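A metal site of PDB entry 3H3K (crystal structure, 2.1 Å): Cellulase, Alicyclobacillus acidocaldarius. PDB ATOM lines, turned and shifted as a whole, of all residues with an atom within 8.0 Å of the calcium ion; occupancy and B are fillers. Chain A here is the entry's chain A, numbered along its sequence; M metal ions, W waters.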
ATOM      1  N   VAL A 152      28.577  36.860  20.519  1.00  0.00           N
ATOM      2  CA  VAL A 152      29.259  35.928  21.424  1.00  0.00           C
ATOM      3  C   VAL A 152      30.710  36.325  21.720  1.00  0.00           C
ATOM      4  O   VAL A 152      31.076  36.441  22.900  1.00  0.00           O
ATOM      5  CB  VAL A 152      29.167  34.446  20.943  1.00  0.00           C
ATOM      6  CG1 VAL A 152      30.091  33.535  21.762  1.00  0.00           C
ATOM      7  CG2 VAL A 152      27.736  33.976  21.006  1.00  0.00           C
ATOM      8  N   ALA A 243      23.185  31.097  22.992  1.00  0.00           N
ATOM      9  CA  ALA A 243      24.553  31.518  23.319  1.00  0.00           C
ATOM     10  C   ALA A 243      24.730  33.031  23.338  1.00  0.00           C
ATOM     11  O   ALA A 243      25.376  33.564  24.240  1.00  0.00           O
ATOM     12  CB  ALA A 243      25.519  30.910  22.338  1.00  0.00           C
ATOM     13  N   THR A 247      25.546  35.044  26.798  1.00  0.00           N
ATOM     14  CA  THR A 247      26.789  35.796  26.905  1.00  0.00           C
ATOM     15  C   THR A 247      26.525  37.298  27.026  1.00  0.00           C
ATOM     16  O   THR A 247      27.264  38.007  27.700  1.00  0.00           O
ATOM     17  CB  THR A 247      27.784  35.496  25.752  1.00  0.00           C
ATOM     18  OG1 THR A 247      27.190  35.822  24.485  1.00  0.00           O
ATOM     19  CG2 THR A 247      28.216  34.040  25.760  1.00  0.00           C
ATOM     20  N   GLY A 301      29.531  29.223  16.415  1.00  0.00           N
ATOM     21  CA  GLY A 301      28.617  28.224  16.922  1.00  0.00           C
ATOM     22  C   GLY A 301      29.257  27.520  18.088  1.00  0.00           C
ATOM     23  O   GLY A 301      30.444  27.683  18.344  1.00  0.00           O
ATOM     24  N   ASP A 302      28.467  26.720  18.791  1.00  0.00           N
ATOM     25  CA  ASP A 302      28.921  26.067  20.015  1.00  0.00           C
ATOM     26  C   ASP A 302      27.833  25.119  20.499  1.00  0.00           C
ATOM     27  O   ASP A 302      26.714  25.539  20.787  1.00  0.00           O
ATOM     28  CB  ASP A 302      29.253  27.126  21.072  1.00  0.00           C
ATOM     29  CG  ASP A 302      29.630  26.526  22.408  1.00  0.00           C
ATOM     30  OD1 ASP A 302      30.175  25.396  22.447  1.00  0.00           O
ATOM     31  OD2 ASP A 302      29.382  27.224  23.428  1.00  0.00           O
ATOM     32  N   ALA A 303      28.168  23.830  20.571  1.00  0.00           N
ATOM     33  CA  ALA A 303      27.200  22.806  20.952  1.00  0.00           C
ATOM     34  C   ALA A 303      26.987  22.739  22.459  1.00  0.00           C
ATOM     35  O   ALA A 303      25.934  22.287  22.920  1.00  0.00           O
ATOM     36  CB  ALA A 303      27.668  21.441  20.429  1.00  0.00           C
ATOM     37  N   GLU A 304      27.970  23.182  23.234  1.00  0.00           N
ATOM     38  CA  GLU A 304      27.887  23.112  24.686  1.00  0.00           C
ATOM     39  C   GLU A 304      27.491  24.462  25.258  1.00  0.00           C
ATOM     40  O   GLU A 304      28.279  25.411  25.201  1.00  0.00           O
ATOM     41  CB  GLU A 304      29.214  22.655  25.300  1.00  0.00           C
ATOM     42  CG  GLU A 304      29.229  22.655  26.829  1.00  0.00           C
ATOM     43  CD  GLU A 304      28.078  21.851  27.422  1.00  0.00           C
ATOM     44  OE1 GLU A 304      28.081  20.607  27.297  1.00  0.00           O
ATOM     45  OE2 GLU A 304      27.152  22.475  27.997  1.00  0.00           O
ATOM     46  N   LEU A 305      26.294  24.552  25.831  1.00  0.00           N
ATOM     47  CA  LEU A 305      25.777  25.835  26.291  1.00  0.00           C
ATOM     48  C   LEU A 305      25.595  25.984  27.809  1.00  0.00           C
ATOM     49  O   LEU A 305      25.180  27.042  28.269  1.00  0.00           O
ATOM     50  CB  LEU A 305      24.462  26.130  25.559  1.00  0.00           C
ATOM     51  CG  LEU A 305      24.646  26.292  24.046  1.00  0.00           C
ATOM     52  CD1 LEU A 305      23.306  26.231  23.328  1.00  0.00           C
ATOM     53  CD2 LEU A 305      25.398  27.583  23.718  1.00  0.00           C
ATOM     54  N   ARG A 306      25.927  24.960  28.583  1.00  0.00           N
ATOM     55  CA  ARG A 306      25.763  25.032  30.043  1.00  0.00           C
ATOM     56  C   ARG A 306      26.762  25.985  30.712  1.00  0.00           C
ATOM     57  O   ARG A 306      26.455  26.574  31.769  1.00  0.00           O
ATOM     58  CB  ARG A 306      25.820  23.638  30.674  1.00  0.00           C
ATOM     59  CG  ARG A 306      24.600  22.809  30.329  1.00  0.00           C
ATOM     60  CD  ARG A 306      24.737  21.404  30.807  1.00  0.00           C
ATOM     61  NE  ARG A 306      25.770  20.702  30.069  1.00  0.00           N
ATOM     62  CZ  ARG A 306      26.226  19.499  30.383  1.00  0.00           C
ATOM     63  NH1 ARG A 306      25.729  18.831  31.410  1.00  0.00           N
ATOM     64  NH2 ARG A 306      27.189  18.948  29.646  1.00  0.00           N
ATOM     65  N   ASP A 307      27.932  26.136  30.104  1.00  0.00           N
ATOM     66  CA  ASP A 307      28.928  27.091  30.599  1.00  0.00           C
ATOM     67  C   ASP A 307      28.451  28.543  30.423  1.00  0.00           C
ATOM     68  O   ASP A 307      28.735  29.382  31.266  1.00  0.00           O
ATOM     69  CB  ASP A 307      30.322  26.869  29.978  1.00  0.00           C
ATOM     70  CG  ASP A 307      30.306  26.812  28.471  1.00  0.00           C
ATOM     71  OD1 ASP A 307      29.649  25.913  27.899  1.00  0.00           O
ATOM     72  OD2 ASP A 307      30.977  27.658  27.832  1.00  0.00           O
ATOM     73  N   GLU A 308      27.696  28.806  29.358  1.00  0.00           N
ATOM     74  CA  GLU A 308      27.097  30.138  29.148  1.00  0.00           C
ATOM     75  C   GLU A 308      26.027  30.458  30.185  1.00  0.00           C
ATOM     76  O   GLU A 308      25.957  31.580  30.694  1.00  0.00           O
ATOM     77  CB  GLU A 308      26.491  30.259  27.749  1.00  0.00           C
ATOM     78  CG  GLU A 308      27.495  30.448  26.619  1.00  0.00           C
ATOM     79  CD  GLU A 308      28.193  29.160  26.204  1.00  0.00           C
ATOM     80  OE1 GLU A 308      27.828  28.081  26.702  1.00  0.00           O
ATOM     81  OE2 GLU A 308      29.127  29.223  25.394  1.00  0.00           O
ATOM     82  N   LEU A 309      25.169  29.484  30.464  1.00  0.00           N
ATOM     83  CA  LEU A 309      24.158  29.626  31.511  1.00  0.00           C
ATOM     84  C   LEU A 309      24.827  29.839  32.863  1.00  0.00           C
ATOM     85  O   LEU A 309      24.361  30.641  33.670  1.00  0.00           O
ATOM     86  CB  LEU A 309      23.252  28.388  31.564  1.00  0.00           C
ATOM     87  CG  LEU A 309      22.104  28.452  32.574  1.00  0.00           C
ATOM     88  CD1 LEU A 309      21.210  29.656  32.282  1.00  0.00           C
ATOM     89  CD2 LEU A 309      21.319  27.135  32.556  1.00  0.00           C
ATOM     90  N   LEU A 337      32.416  20.738  33.204  1.00  0.00           N
ATOM     91  CA  LEU A 337      32.676  21.655  32.098  1.00  0.00           C
ATOM     92  C   LEU A 337      34.135  22.063  32.135  1.00  0.00           C
ATOM     93  O   LEU A 337      34.731  22.124  33.205  1.00  0.00           O
ATOM     94  CB  LEU A 337      31.802  22.912  32.219  1.00  0.00           C
ATOM     95  CG  LEU A 337      30.286  22.731  32.074  1.00  0.00           C
ATOM     96  CD1 LEU A 337      29.552  24.018  32.427  1.00  0.00           C
ATOM     97  CD2 LEU A 337      29.944  22.291  30.659  1.00  0.00           C
ATOM     98  N   PRO A 338      34.738  22.341  30.972  1.00  0.00           N
ATOM     99  CA  PRO A 338      36.063  22.958  31.015  1.00  0.00           C
ATOM    100  C   PRO A 338      35.937  24.398  31.542  1.00  0.00           C
ATOM    101  O   PRO A 338      34.982  25.103  31.207  1.00  0.00           O
ATOM    102  CB  PRO A 338      36.517  22.933  29.554  1.00  0.00           C
ATOM    103  CG  PRO A 338      35.261  22.890  28.763  1.00  0.00           C
ATOM    104  CD  PRO A 338      34.275  22.124  29.588  1.00  0.00           C
ATOM    105  N   GLY A 342      36.742  31.514  27.104  1.00  0.00           N
ATOM    106  CA  GLY A 342      36.068  31.798  25.846  1.00  0.00           C
ATOM    107  C   GLY A 342      36.941  31.656  24.616  1.00  0.00           C
ATOM    108  O   GLY A 342      38.113  31.304  24.734  1.00  0.00           O
ATOM    109  N   TRP A 343      36.401  31.967  23.439  1.00  0.00           N
ATOM    110  CA  TRP A 343      35.057  32.546  23.306  1.00  0.00           C
ATOM    111  C   TRP A 343      33.907  31.534  23.442  1.00  0.00           C
ATOM    112  O   TRP A 343      32.785  31.924  23.736  1.00  0.00           O
ATOM    113  CB  TRP A 343      34.934  33.308  21.963  1.00  0.00           C
ATOM    114  CG  TRP A 343      35.262  32.460  20.771  1.00  0.00           C
ATOM    115  CD1 TRP A 343      36.471  32.358  20.151  1.00  0.00           C
ATOM    116  CD2 TRP A 343      34.373  31.573  20.074  1.00  0.00           C
ATOM    117  NE1 TRP A 343      36.379  31.466  19.103  1.00  0.00           N
ATOM    118  CE2 TRP A 343      35.110  30.972  19.035  1.00  0.00           C
ATOM    119  CE3 TRP A 343      33.012  31.241  20.224  1.00  0.00           C
ATOM    120  CZ2 TRP A 343      34.541  30.054  18.142  1.00  0.00           C
ATOM    121  CZ3 TRP A 343      32.460  30.324  19.345  1.00  0.00           C
ATOM    122  CH2 TRP A 343      33.225  29.743  18.312  1.00  0.00           C
ATOM    123  N   ALA A 344      34.204  30.240  23.255  1.00  0.00           N
ATOM    124  CA  ALA A 344      33.167  29.195  23.249  1.00  0.00           C
ATOM    125  C   ALA A 344      32.985  28.524  24.606  1.00  0.00           C
ATOM    126  O   ALA A 344      31.864  28.173  24.988  1.00  0.00           O
ATOM    127  CB  ALA A 344      33.492  28.133  22.200  1.00  0.00           C
ATOM    128  N   ASP A 345      34.088  28.348  25.328  1.00  0.00           N
ATOM    129  CA  ASP A 345      34.100  27.711  26.639  1.00  0.00           C
ATOM    130  C   ASP A 345      34.388  28.783  27.690  1.00  0.00           C
ATOM    131  O   ASP A 345      35.552  29.164  27.902  1.00  0.00           O
ATOM    132  CB  ASP A 345      35.171  26.626  26.666  1.00  0.00           C
ATOM    133  CG  ASP A 345      34.909  25.545  25.628  1.00  0.00           C
ATOM    134  OD1 ASP A 345      35.579  25.579  24.550  1.00  0.00           O
ATOM    135  OD2 ASP A 345      34.007  24.705  25.845  1.00  0.00           O
ATOM    136  N   VAL A 346      33.337  29.271  28.344  1.00  0.00           N
ATOM    137  CA  VAL A 346      33.380  30.483  29.152  1.00  0.00           C
ATOM    138  C   VAL A 346      33.130  30.265  30.660  1.00  0.00           C
ATOM    139  O   VAL A 346      32.872  31.232  31.368  1.00  0.00           O
ATOM    140  CB  VAL A 346      32.312  31.497  28.640  1.00  0.00           C
ATOM    141  CG1 VAL A 346      32.637  31.961  27.240  1.00  0.00           C
ATOM    142  CG2 VAL A 346      30.908  30.904  28.715  1.00  0.00           C
ATOM    143  N   ALA A 347      33.209  29.020  31.143  1.00  0.00           N
ATOM    144  CA  ALA A 347      32.851  28.735  32.545  1.00  0.00           C
ATOM    145  C   ALA A 347      33.695  29.496  33.572  1.00  0.00           C
ATOM    146  O   ALA A 347      33.179  29.890  34.601  1.00  0.00           O
ATOM    147  CB  ALA A 347      32.904  27.249  32.820  1.00  0.00           C
HETATM  148 CA    CA M   1      29.943  26.966  25.602  1.00  0.00          CA
HETATM  149  O   HOH W   1      31.355  25.312  24.897  1.00  0.00           O
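The side-chain carboxylate (OD2) of Asp 307 sits close to the backbone NH (N) of Val 346 (2.9 Å). NH2 of Arg 306 lies within salt-bridge range of OE1 of Glu 304, at 3.0 Å.
Of the 20 residues printed, 5 come within 4 Å of the calcium ion. The nearest printed residue that does not touch the calcium ion is Asp 345 (4.3 Å).
The calcium ion is bound by the side-chain carboxylate (OD2) of Asp 302 (2.3 Å), water W1 (2.3 Å), the backbone carbonyl oxygen (O) of Glu 304 (2.3 Å), the backbone carbonyl oxygen (O) of Ala 344 (2.4 Å), the side-chain carboxylate (OE2) of Glu 308 (2.4 Å), the side-chain carboxylate (OD1) of Asp 307 (2.5 Å), the side-chain carboxylate (OD2) of Asp 307 (2.6 Å) and the side-chain carboxylate (OE1) of Glu 308 (2.6 Å).
Water W1 lies within hydrogen-bond range of the side-chain carboxylate (OD1) of Asp 302 (2.7 Å) and the side-chain carboxylate (OD2) of Asp 345 (2.9 Å).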
